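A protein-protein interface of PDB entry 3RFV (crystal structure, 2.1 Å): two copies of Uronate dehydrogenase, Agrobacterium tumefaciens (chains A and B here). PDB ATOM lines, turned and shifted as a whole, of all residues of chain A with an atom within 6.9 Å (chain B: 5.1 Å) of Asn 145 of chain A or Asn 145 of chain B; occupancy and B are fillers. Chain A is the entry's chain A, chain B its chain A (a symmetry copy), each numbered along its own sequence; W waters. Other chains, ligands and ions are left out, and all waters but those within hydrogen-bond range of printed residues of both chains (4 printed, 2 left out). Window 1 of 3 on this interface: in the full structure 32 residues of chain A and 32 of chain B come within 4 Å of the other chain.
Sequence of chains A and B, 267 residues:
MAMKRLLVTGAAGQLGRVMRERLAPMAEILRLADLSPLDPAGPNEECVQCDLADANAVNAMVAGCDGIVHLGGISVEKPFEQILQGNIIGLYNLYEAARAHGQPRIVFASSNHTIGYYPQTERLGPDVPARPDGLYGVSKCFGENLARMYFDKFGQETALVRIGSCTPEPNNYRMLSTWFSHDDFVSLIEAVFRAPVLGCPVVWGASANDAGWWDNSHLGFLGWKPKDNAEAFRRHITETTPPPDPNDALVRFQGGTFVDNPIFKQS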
ATOM      1  N   PHE A 108     -15.039   6.169   1.252  1.00  0.00           N
ATOM      2  CA  PHE A 108     -13.886   7.038   1.118  1.00  0.00           C
ATOM      3  C   PHE A 108     -14.342   8.417   0.664  1.00  0.00           C
ATOM      4  O   PHE A 108     -14.988   8.547  -0.376  1.00  0.00           O
ATOM      5  CB  PHE A 108     -12.884   6.450   0.119  1.00  0.00           C
ATOM      6  CG  PHE A 108     -11.711   7.354  -0.176  1.00  0.00           C
ATOM      7  CD1 PHE A 108     -10.991   7.940   0.852  1.00  0.00           C
ATOM      8  CD2 PHE A 108     -11.325   7.608  -1.484  1.00  0.00           C
ATOM      9  CE1 PHE A 108      -9.913   8.772   0.578  1.00  0.00           C
ATOM     10  CE2 PHE A 108     -10.250   8.431  -1.762  1.00  0.00           C
ATOM     11  CZ  PHE A 108      -9.541   9.009  -0.730  1.00  0.00           C
ATOM     12  N   PRO A 129     -11.280  10.143 -17.491  1.00  0.00           N
ATOM     13  CA  PRO A 129      -9.895  10.212 -17.021  1.00  0.00           C
ATOM     14  C   PRO A 129      -9.740  11.327 -15.982  1.00  0.00           C
ATOM     15  O   PRO A 129     -10.363  12.400 -16.113  1.00  0.00           O
ATOM     16  CB  PRO A 129      -9.116  10.562 -18.293  1.00  0.00           C
ATOM     17  CG  PRO A 129      -9.988  10.119 -19.408  1.00  0.00           C
ATOM     18  CD  PRO A 129     -11.388  10.353 -18.943  1.00  0.00           C
ATOM     19  N   ALA A 130      -8.927  11.071 -14.962  1.00  0.00           N
ATOM     20  CA  ALA A 130      -8.682  12.043 -13.909  1.00  0.00           C
ATOM     21  C   ALA A 130      -8.050  13.315 -14.481  1.00  0.00           C
ATOM     22  O   ALA A 130      -7.234  13.256 -15.391  1.00  0.00           O
ATOM     23  CB  ALA A 130      -7.771  11.441 -12.842  1.00  0.00           C
ATOM     24  N   ARG A 131      -8.428  14.457 -13.935  1.00  0.00           N
ATOM     25  CA  ARG A 131      -7.740  15.707 -14.232  1.00  0.00           C
ATOM     26  C   ARG A 131      -7.618  16.506 -12.938  1.00  0.00           C
ATOM     27  O   ARG A 131      -8.266  17.534 -12.768  1.00  0.00           O
ATOM     28  CB  ARG A 131      -8.476  16.490 -15.333  1.00  0.00           C
ATOM     29  CG  ARG A 131      -8.350  15.815 -16.715  1.00  0.00           C
ATOM     30  CD  ARG A 131      -8.980  16.630 -17.820  1.00  0.00           C
ATOM     31  NE  ARG A 131      -8.241  17.859 -18.104  1.00  0.00           N
ATOM     32  CZ  ARG A 131      -8.686  18.808 -18.924  1.00  0.00           C
ATOM     33  NH1 ARG A 131      -9.861  18.655 -19.526  1.00  0.00           N
ATOM     34  NH2 ARG A 131      -7.967  19.905 -19.141  1.00  0.00           N
ATOM     35  N   PRO A 132      -6.775  16.014 -12.016  1.00  0.00           N
ATOM     36  CA  PRO A 132      -6.639  16.598 -10.679  1.00  0.00           C
ATOM     37  C   PRO A 132      -6.109  18.028 -10.769  1.00  0.00           C
ATOM     38  O   PRO A 132      -5.275  18.323 -11.631  1.00  0.00           O
ATOM     39  CB  PRO A 132      -5.638  15.671  -9.974  1.00  0.00           C
ATOM     40  CG  PRO A 132      -4.911  14.967 -11.061  1.00  0.00           C
ATOM     41  CD  PRO A 132      -5.780  14.963 -12.288  1.00  0.00           C
ATOM     42  N   GLY A 134      -4.551  19.861  -8.366  1.00  0.00           N
ATOM     43  CA  GLY A 134      -3.425  20.171  -7.495  1.00  0.00           C
ATOM     44  C   GLY A 134      -2.913  18.919  -6.794  1.00  0.00           C
ATOM     45  O   GLY A 134      -3.372  17.812  -7.086  1.00  0.00           O
ATOM     46  N   GLY A 137      -5.856  17.063  -5.094  1.00  0.00           N
ATOM     47  CA  GLY A 137      -6.604  16.241  -6.032  1.00  0.00           C
ATOM     48  C   GLY A 137      -5.835  14.971  -6.390  1.00  0.00           C
ATOM     49  O   GLY A 137      -6.404  13.879  -6.432  1.00  0.00           O
ATOM     50  N   VAL A 138      -4.541  15.120  -6.659  1.00  0.00           N
ATOM     51  CA  VAL A 138      -3.698  13.984  -7.004  1.00  0.00           C
ATOM     52  C   VAL A 138      -3.722  12.940  -5.893  1.00  0.00           C
ATOM     53  O   VAL A 138      -3.768  11.747  -6.169  1.00  0.00           O
ATOM     54  CB  VAL A 138      -2.247  14.430  -7.282  1.00  0.00           C
ATOM     55  CG1 VAL A 138      -1.299  13.218  -7.385  1.00  0.00           C
ATOM     56  CG2 VAL A 138      -2.195  15.250  -8.561  1.00  0.00           C
ATOM     57  N   SER A 139      -3.703  13.390  -4.641  1.00  0.00           N
ATOM     58  CA  SER A 139      -3.703  12.471  -3.507  1.00  0.00           C
ATOM     59  C   SER A 139      -5.041  11.768  -3.372  1.00  0.00           C
ATOM     60  O   SER A 139      -5.101  10.615  -2.934  1.00  0.00           O
ATOM     61  CB  SER A 139      -3.352  13.196  -2.198  1.00  0.00           C
ATOM     62  OG  SER A 139      -4.466  13.928  -1.702  1.00  0.00           O
ATOM     63  N   LYS A 140      -6.123  12.446  -3.745  1.00  0.00           N
ATOM     64  CA  LYS A 140      -7.422  11.779  -3.743  1.00  0.00           C
ATOM     65  C   LYS A 140      -7.480  10.718  -4.859  1.00  0.00           C
ATOM     66  O   LYS A 140      -8.040   9.643  -4.665  1.00  0.00           O
ATOM     67  CB  LYS A 140      -8.578  12.778  -3.823  1.00  0.00           C
ATOM     68  CG  LYS A 140      -8.740  13.630  -2.555  1.00  0.00           C
ATOM     69  CD  LYS A 140      -9.055  12.759  -1.324  1.00  0.00           C
ATOM     70  CE  LYS A 140      -9.344  13.634  -0.092  1.00  0.00           C
ATOM     71  NZ  LYS A 140      -9.754  12.850   1.110  1.00  0.00           N
ATOM     72  N   CYS A 141      -6.864  11.010  -6.002  1.00  0.00           N
ATOM     73  CA  CYS A 141      -6.697  10.006  -7.054  1.00  0.00           C
ATOM     74  C   CYS A 141      -5.921   8.801  -6.522  1.00  0.00           C
ATOM     75  O   CYS A 141      -6.260   7.662  -6.829  1.00  0.00           O
ATOM     76  CB  CYS A 141      -5.966  10.585  -8.263  1.00  0.00           C
ATOM     77  SG  CYS A 141      -6.955  11.776  -9.245  1.00  0.00           S
ATOM     78  N   PHE A 142      -4.876   9.059  -5.735  1.00  0.00           N
ATOM     79  CA  PHE A 142      -4.088   7.982  -5.132  1.00  0.00           C
ATOM     80  C   PHE A 142      -4.966   7.074  -4.273  1.00  0.00           C
ATOM     81  O   PHE A 142      -4.897   5.844  -4.389  1.00  0.00           O
ATOM     82  CB  PHE A 142      -2.904   8.523  -4.306  1.00  0.00           C
ATOM     83  CG  PHE A 142      -2.187   7.456  -3.515  1.00  0.00           C
ATOM     84  CD1 PHE A 142      -1.140   6.737  -4.077  1.00  0.00           C
ATOM     85  CD2 PHE A 142      -2.583   7.153  -2.223  1.00  0.00           C
ATOM     86  CE1 PHE A 142      -0.494   5.744  -3.360  1.00  0.00           C
ATOM     87  CE2 PHE A 142      -1.935   6.151  -1.496  1.00  0.00           C
ATOM     88  CZ  PHE A 142      -0.898   5.454  -2.062  1.00  0.00           C
ATOM     89  N   GLY A 143      -5.781   7.675  -3.414  1.00  0.00           N
ATOM     90  CA  GLY A 143      -6.716   6.921  -2.605  1.00  0.00           C
ATOM     91  C   GLY A 143      -7.635   6.060  -3.461  1.00  0.00           C
ATOM     92  O   GLY A 143      -7.916   4.912  -3.129  1.00  0.00           O
ATOM     93  N   GLU A 144      -8.112   6.620  -4.567  1.00  0.00           N
ATOM     94  CA  GLU A 144      -8.984   5.881  -5.473  1.00  0.00           C
ATOM     95  C   GLU A 144      -8.276   4.697  -6.129  1.00  0.00           C
ATOM     96  O   GLU A 144      -8.840   3.602  -6.216  1.00  0.00           O
ATOM     97  CB  GLU A 144      -9.544   6.804  -6.567  1.00  0.00           C
ATOM     98  CG  GLU A 144     -10.494   7.879  -6.062  1.00  0.00           C
ATOM     99  CD  GLU A 144     -11.220   8.596  -7.199  1.00  0.00           C
ATOM    100  OE1 GLU A 144     -10.980   8.269  -8.376  1.00  0.00           O
ATOM    101  OE2 GLU A 144     -12.044   9.481  -6.909  1.00  0.00           O
ATOM    102  N   ASN A 145      -7.061   4.921  -6.622  1.00  0.00           N
ATOM    103  CA  ASN A 145      -6.323   3.861  -7.288  1.00  0.00           C
ATOM    104  C   ASN A 145      -5.937   2.769  -6.297  1.00  0.00           C
ATOM    105  O   ASN A 145      -5.993   1.575  -6.617  1.00  0.00           O
ATOM    106  CB  ASN A 145      -5.077   4.415  -7.987  1.00  0.00           C
ATOM    107  CG  ASN A 145      -5.426   5.400  -9.111  1.00  0.00           C
ATOM    108  OD1 ASN A 145      -6.458   5.263  -9.772  1.00  0.00           O
ATOM    109  ND2 ASN A 145      -4.567   6.386  -9.329  1.00  0.00           N
ATOM    110  N   LEU A 146      -5.559   3.183  -5.091  1.00  0.00           N
ATOM    111  CA  LEU A 146      -5.197   2.244  -4.036  1.00  0.00           C
ATOM    112  C   LEU A 146      -6.400   1.384  -3.644  1.00  0.00           C
ATOM    113  O   LEU A 146      -6.302   0.158  -3.604  1.00  0.00           O
ATOM    114  CB  LEU A 146      -4.659   2.977  -2.807  1.00  0.00           C
ATOM    115  CG  LEU A 146      -4.096   2.060  -1.710  1.00  0.00           C
ATOM    116  CD1 LEU A 146      -2.711   1.608  -2.109  1.00  0.00           C
ATOM    117  CD2 LEU A 146      -4.069   2.747  -0.352  1.00  0.00           C
ATOM    118  N   ALA A 147      -7.529   2.032  -3.356  1.00  0.00           N
ATOM    119  CA  ALA A 147      -8.773   1.321  -3.061  1.00  0.00           C
ATOM    120  C   ALA A 147      -9.135   0.326  -4.162  1.00  0.00           C
ATOM    121  O   ALA A 147      -9.586  -0.787  -3.876  1.00  0.00           O
ATOM    122  CB  ALA A 147      -9.916   2.301  -2.856  1.00  0.00           C
ATOM    123  N   ARG A 148      -8.966   0.730  -5.419  1.00  0.00           N
ATOM    124  CA  ARG A 148      -9.314  -0.156  -6.530  1.00  0.00           C
ATOM    125  C   ARG A 148      -8.438  -1.410  -6.533  1.00  0.00           C
ATOM    126  O   ARG A 148      -8.938  -2.512  -6.733  1.00  0.00           O
ATOM    127  CB  ARG A 148      -9.234   0.557  -7.884  1.00  0.00           C
ATOM    128  CG  ARG A 148      -9.570  -0.356  -9.087  1.00  0.00           C
ATOM    129  CD  ARG A 148     -11.047  -0.772  -9.107  1.00  0.00           C
ATOM    130  NE  ARG A 148     -11.254  -2.088  -9.724  1.00  0.00           N
ATOM    131  CZ  ARG A 148     -12.400  -2.494 -10.272  1.00  0.00           C
ATOM    132  NH1 ARG A 148     -13.446  -1.682 -10.325  1.00  0.00           N
ATOM    133  NH2 ARG A 148     -12.498  -3.713 -10.789  1.00  0.00           N
ATOM    134  N   MET A 149      -7.136  -1.231  -6.325  1.00  0.00           N
ATOM    135  CA  MET A 149      -6.206  -2.355  -6.251  1.00  0.00           C
ATOM    136  C   MET A 149      -6.592  -3.321  -5.124  1.00  0.00           C
ATOM    137  O   MET A 149      -6.608  -4.541  -5.328  1.00  0.00           O
ATOM    138  CB  MET A 149      -4.756  -1.860  -6.097  1.00  0.00           C
ATOM    139  CG  MET A 149      -3.693  -2.963  -6.114  1.00  0.00           C
ATOM    140  SD  MET A 149      -3.410  -3.642  -4.451  1.00  0.00           S
ATOM    141  CE  MET A 149      -2.485  -2.289  -3.691  1.00  0.00           C
ATOM    142  N   TYR A 150      -6.918  -2.782  -3.949  1.00  0.00           N
ATOM    143  CA  TYR A 150      -7.369  -3.609  -2.833  1.00  0.00           C
ATOM    144  C   TYR A 150      -8.650  -4.360  -3.143  1.00  0.00           C
ATOM    145  O   TYR A 150      -8.828  -5.504  -2.693  1.00  0.00           O
ATOM    146  CB  TYR A 150      -7.497  -2.807  -1.521  1.00  0.00           C
ATOM    147  CG  TYR A 150      -6.168  -2.672  -0.815  1.00  0.00           C
ATOM    148  CD1 TYR A 150      -5.811  -3.533   0.221  1.00  0.00           C
ATOM    149  CD2 TYR A 150      -5.253  -1.705  -1.208  1.00  0.00           C
ATOM    150  CE1 TYR A 150      -4.583  -3.414   0.858  1.00  0.00           C
ATOM    151  CE2 TYR A 150      -4.035  -1.575  -0.584  1.00  0.00           C
ATOM    152  CZ  TYR A 150      -3.699  -2.434   0.450  1.00  0.00           C
ATOM    153  OH  TYR A 150      -2.473  -2.291   1.055  1.00  0.00           O
ATOM    154  N   LEU A 160     -16.100   5.197  -3.586  1.00  0.00           N
ATOM    155  CA  LEU A 160     -15.207   6.319  -3.870  1.00  0.00           C
ATOM    156  C   LEU A 160     -16.052   7.565  -4.105  1.00  0.00           C
ATOM    157  O   LEU A 160     -16.443   7.868  -5.237  1.00  0.00           O
ATOM    158  CB  LEU A 160     -14.329   6.028  -5.096  1.00  0.00           C
ATOM    159  CG  LEU A 160     -13.508   4.740  -5.071  1.00  0.00           C
ATOM    160  CD1 LEU A 160     -12.832   4.511  -6.414  1.00  0.00           C
ATOM    161  CD2 LEU A 160     -12.486   4.763  -3.938  1.00  0.00           C
ATOM    162  N   ALA B 130      -8.054   3.082 -14.542  1.00  0.00           N
ATOM    163  CA  ALA B 130      -6.915   2.344 -14.019  1.00  0.00           C
ATOM    164  C   ALA B 130      -7.378   1.101 -13.255  1.00  0.00           C
ATOM    165  O   ALA B 130      -8.392   1.126 -12.571  1.00  0.00           O
ATOM    166  CB  ALA B 130      -6.084   3.242 -13.104  1.00  0.00           C
ATOM    167  N   PRO B 132      -4.749  -0.937 -11.275  1.00  0.00           N
ATOM    168  CA  PRO B 132      -3.373  -1.265 -10.891  1.00  0.00           C
ATOM    169  C   PRO B 132      -3.328  -2.597 -10.145  1.00  0.00           C
ATOM    170  O   PRO B 132      -4.245  -2.907  -9.379  1.00  0.00           O
ATOM    171  CB  PRO B 132      -2.958  -0.098  -9.983  1.00  0.00           C
ATOM    172  CG  PRO B 132      -4.226   0.514  -9.513  1.00  0.00           C
ATOM    173  CD  PRO B 132      -5.308   0.188 -10.506  1.00  0.00           C
ATOM    174  N   VAL B 138       0.056   1.149  -8.618  1.00  0.00           N
ATOM    175  CA  VAL B 138      -0.565   2.322  -8.021  1.00  0.00           C
ATOM    176  C   VAL B 138       0.373   3.521  -8.090  1.00  0.00           C
ATOM    177  O   VAL B 138      -0.064   4.633  -8.364  1.00  0.00           O
ATOM    178  CB  VAL B 138      -0.977   2.052  -6.557  1.00  0.00           C
ATOM    179  CG1 VAL B 138      -1.386   3.355  -5.842  1.00  0.00           C
ATOM    180  CG2 VAL B 138      -2.117   1.048  -6.518  1.00  0.00           C
ATOM    181  N   CYS B 141       0.425   4.928 -11.500  1.00  0.00           N
ATOM    182  CA  CYS B 141      -0.775   5.757 -11.623  1.00  0.00           C
ATOM    183  C   CYS B 141      -0.538   7.134 -11.002  1.00  0.00           C
ATOM    184  O   CYS B 141      -0.957   8.144 -11.558  1.00  0.00           O
ATOM    185  CB  CYS B 141      -1.977   5.098 -10.950  1.00  0.00           C
ATOM    186  SG  CYS B 141      -2.627   3.630 -11.835  1.00  0.00           S
ATOM    187  N   PHE B 142       0.125   7.165  -9.845  1.00  0.00           N
ATOM    188  CA  PHE B 142       0.448   8.430  -9.182  1.00  0.00           C
ATOM    189  C   PHE B 142       1.279   9.330 -10.094  1.00  0.00           C
ATOM    190  O   PHE B 142       0.977  10.520 -10.244  1.00  0.00           O
ATOM    191  CB  PHE B 142       1.170   8.212  -7.838  1.00  0.00           C
ATOM    192  CG  PHE B 142       1.689   9.488  -7.221  1.00  0.00           C
ATOM    193  CD1 PHE B 142       0.887  10.248  -6.380  1.00  0.00           C
ATOM    194  CD2 PHE B 142       2.966   9.940  -7.510  1.00  0.00           C
ATOM    195  CE1 PHE B 142       1.355  11.430  -5.830  1.00  0.00           C
ATOM    196  CE2 PHE B 142       3.441  11.132  -6.958  1.00  0.00           C
ATOM    197  CZ  PHE B 142       2.640  11.869  -6.123  1.00  0.00           C
ATOM    198  N   GLY B 143       2.323   8.767 -10.694  1.00  0.00           N
ATOM    199  CA  GLY B 143       3.136   9.501 -11.641  1.00  0.00           C
ATOM    200  C   GLY B 143       2.301  10.065 -12.782  1.00  0.00           C
ATOM    201  O   GLY B 143       2.498  11.198 -13.210  1.00  0.00           O
ATOM    202  N   GLU B 144       1.366   9.266 -13.284  1.00  0.00           N
ATOM    203  CA  GLU B 144       0.492   9.709 -14.366  1.00  0.00           C
ATOM    204  C   GLU B 144      -0.422  10.859 -13.944  1.00  0.00           C
ATOM    205  O   GLU B 144      -0.587  11.830 -14.688  1.00  0.00           O
ATOM    206  CB  GLU B 144      -0.366   8.547 -14.887  1.00  0.00           C
ATOM    207  CG  GLU B 144       0.418   7.443 -15.581  1.00  0.00           C
ATOM    208  CD  GLU B 144      -0.490   6.449 -16.304  1.00  0.00           C
ATOM    209  OE1 GLU B 144      -1.724   6.608 -16.259  1.00  0.00           O
ATOM    210  OE2 GLU B 144       0.038   5.514 -16.931  1.00  0.00           O
ATOM    211  N   ASN B 145      -1.042  10.735 -12.773  1.00  0.00           N
ATOM    212  CA  ASN B 145      -1.952  11.766 -12.303  1.00  0.00           C
ATOM    213  C   ASN B 145      -1.194  13.052 -11.992  1.00  0.00           C
ATOM    214  O   ASN B 145      -1.673  14.155 -12.281  1.00  0.00           O
ATOM    215  CB  ASN B 145      -2.729  11.291 -11.071  1.00  0.00           C
ATOM    216  CG  ASN B 145      -3.638  10.093 -11.379  1.00  0.00           C
ATOM    217  OD1 ASN B 145      -4.161   9.968 -12.488  1.00  0.00           O
ATOM    218  ND2 ASN B 145      -3.828   9.221 -10.400  1.00  0.00           N
ATOM    219  N   LEU B 146      -0.005  12.903 -11.414  1.00  0.00           N
ATOM    220  CA  LEU B 146       0.841  14.047 -11.094  1.00  0.00           C
ATOM    221  C   LEU B 146       1.267  14.775 -12.370  1.00  0.00           C
ATOM    222  O   LEU B 146       1.115  15.992 -12.472  1.00  0.00           O
ATOM    223  CB  LEU B 146       2.076  13.613 -10.304  1.00  0.00           C
ATOM    224  CG  LEU B 146       2.938  14.772  -9.778  1.00  0.00           C
ATOM    225  CD1 LEU B 146       2.288  15.348  -8.543  1.00  0.00           C
ATOM    226  CD2 LEU B 146       4.365  14.331  -9.481  1.00  0.00           C
ATOM    227  N   ALA B 147       1.802  14.027 -13.335  1.00  0.00           N
ATOM    228  CA  ALA B 147       2.161  14.587 -14.636  1.00  0.00           C
ATOM    229  C   ALA B 147       0.989  15.323 -15.283  1.00  0.00           C
ATOM    230  O   ALA B 147       1.170  16.390 -15.877  1.00  0.00           O
ATOM    231  CB  ALA B 147       2.664  13.499 -15.570  1.00  0.00           C
ATOM    232  N   ARG B 148      -0.207  14.745 -15.195  1.00  0.00           N
ATOM    233  CA  ARG B 148      -1.375  15.374 -15.811  1.00  0.00           C
ATOM    234  C   ARG B 148      -1.684  16.724 -15.162  1.00  0.00           C
ATOM    235  O   ARG B 148      -1.970  17.693 -15.857  1.00  0.00           O
ATOM    236  CB  ARG B 148      -2.609  14.466 -15.771  1.00  0.00           C
ATOM    237  CG  ARG B 148      -3.873  15.108 -16.390  1.00  0.00           C
ATOM    238  CD  ARG B 148      -3.747  15.295 -17.907  1.00  0.00           C
ATOM    239  NE  ARG B 148      -4.514  16.446 -18.399  1.00  0.00           N
ATOM    240  CZ  ARG B 148      -4.949  16.584 -19.653  1.00  0.00           C
ATOM    241  NH1 ARG B 148      -4.737  15.631 -20.548  1.00  0.00           N
ATOM    242  NH2 ARG B 148      -5.620  17.673 -20.010  1.00  0.00           N
ATOM    243  N   MET B 149      -1.636  16.774 -13.832  1.00  0.00           N
ATOM    244  CA  MET B 149      -1.858  18.017 -13.099  1.00  0.00           C
ATOM    245  C   MET B 149      -0.840  19.091 -13.508  1.00  0.00           C
ATOM    246  O   MET B 149      -1.215  20.245 -13.750  1.00  0.00           O
ATOM    247  CB  MET B 149      -1.837  17.772 -11.580  1.00  0.00           C
ATOM    248  CG  MET B 149      -2.163  19.000 -10.723  1.00  0.00           C
ATOM    249  SD  MET B 149      -0.673  19.979 -10.367  1.00  0.00           S
ATOM    250  CE  MET B 149       0.139  18.920  -9.150  1.00  0.00           C
HETATM  251  O   HOH W   1      -5.070  17.494 -14.290  1.00  0.00           O
HETATM  252  O   HOH W   2      -2.260   6.725  -7.681  1.00  0.00           O
HETATM  253  O   HOH W   3      -2.488   9.500  -7.894  1.00  0.00           O
HETATM  254  O   HOH W   4      -6.999  -2.509  -9.622  1.00  0.00           O
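The side-chain amide nitrogen (ND2) of Asn 145 of chain A sits close to the side-chain amide nitrogen (ND2) of Asn 145 of chain B (3.1 Å).
NH2 of Arg 148 of chain B lies close to NE of Arg 131 of chain A (3.2 Å).
O of Gly 137 of chain A sits at hydrogen-bond distance from SG of Cys 141 of chain A.
O of Cys 141 of chain A lies within hydrogen-bond range of ND2 of Asn 145 of chain A (3.3 Å).
O of Cys 141 of chain B lies within hydrogen-bond range of ND2 of Asn 145 of chain B (3.3 Å).
CG of Arg 148 of chain B touches O of Ala 130 of chain A, 3.97 Å away.
Pro 132 of chain A touches Met 149 of chain B.
Met 149 of chain B touches Gly 134 of chain A.
Phe 142 of chain B touches Val 138 of chain A (CE1 to CG1, 3.6 Å).
Val 138 of chain A touches Asn 145 of chain B.
Asn 145 of chain B touches Cys 141 of chain A (ND2 to CB, 3.3 Å).
Val 138 of chain B touches Phe 142 of chain A (CG1 to CE1, 3.6 Å).
Asn 145 of chain A touches Pro 132 of chain B (O to CG, 3.6 Å).
Asn 145 of chain A touches Val 138 of chain B (O to CG2, 3.9 Å).
CB of Met 149 of chain A touches CG2 of Val 138 of chain B, at 3.9 Å.
Asn 145 of chain A touches five residues of chain B.
Of chain A, only Ala 130, Pro 132, Val 138, Cys 141 and Asn 145 come within 4 Å of Asn 145 of chain B.
Of the printed residues of chain A, Phe 142 of chain B touches Val 138 (3.6 Å).
Of the printed residues of chain B, Ala 130 of chain A touches Asn 145 and Arg 148.
Of the printed residues of chain B, Val 138 of chain A touches Phe 142, Asn 145 and Met 149.
Of the printed residues of chain A, Cys 141 of chain B touches Asn 145.
The nearest residue of chain A that does not touch Asn 145 of chain B is Phe 142 of chain A (4.8 Å).
Of the 21 printed residues of chain A, 10 touch a printed residue of chain B.
Hydrophobic or aromatic side chains of chain A within 4 Å of the printed part of chain B: Ala 130, Pro 132, Val 138, Phe 142 and Met 149.
Among the printed residues, 19 pairs touch across the chains.
Pro 132 of chain A touches Asn 145 of chain B, and with the chains exchanged Asn 145 of chain A touches Pro 132 of chain B.
Pro 132 of chain A touches Met 149 of chain B, and with the chains exchanged Met 149 of chain A touches Pro 132 of chain B.
Val 138 of chain A touches Phe 142 of chain B, and with the chains exchanged Phe 142 of chain A touches Val 138 of chain B.
Asn 145 of chain B touches its own counterpart, Asn 145 of chain A.
12 positions are printed for both chains.
Water W4 lies within hydrogen-bond range of O of Pro 132 of chain B and O of Arg 148 of chain A.
Water W1 bridges the backbone carbonyl oxygen of Pro 132 of chain A (2.8 Å) and the backbone carbonyl oxygen of Arg 148 of chain B (3.5 Å).
Water W2 lies within hydrogen-bond range of the side-chain amide nitrogen of Asn 145 of chain A, the backbone carbonyl oxygen of Val 138 of chain B and the backbone NH of Phe 142 of chain B.
Water W3 lies within hydrogen-bond range of the side-chain amide nitrogen (ND2) of Asn 145 of chain B (2.9 Å), the backbone carbonyl oxygen (O) of Val 138 of chain A (3.1 Å) and the backbone NH (N) of Phe 142 of chain A (3.2 Å).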
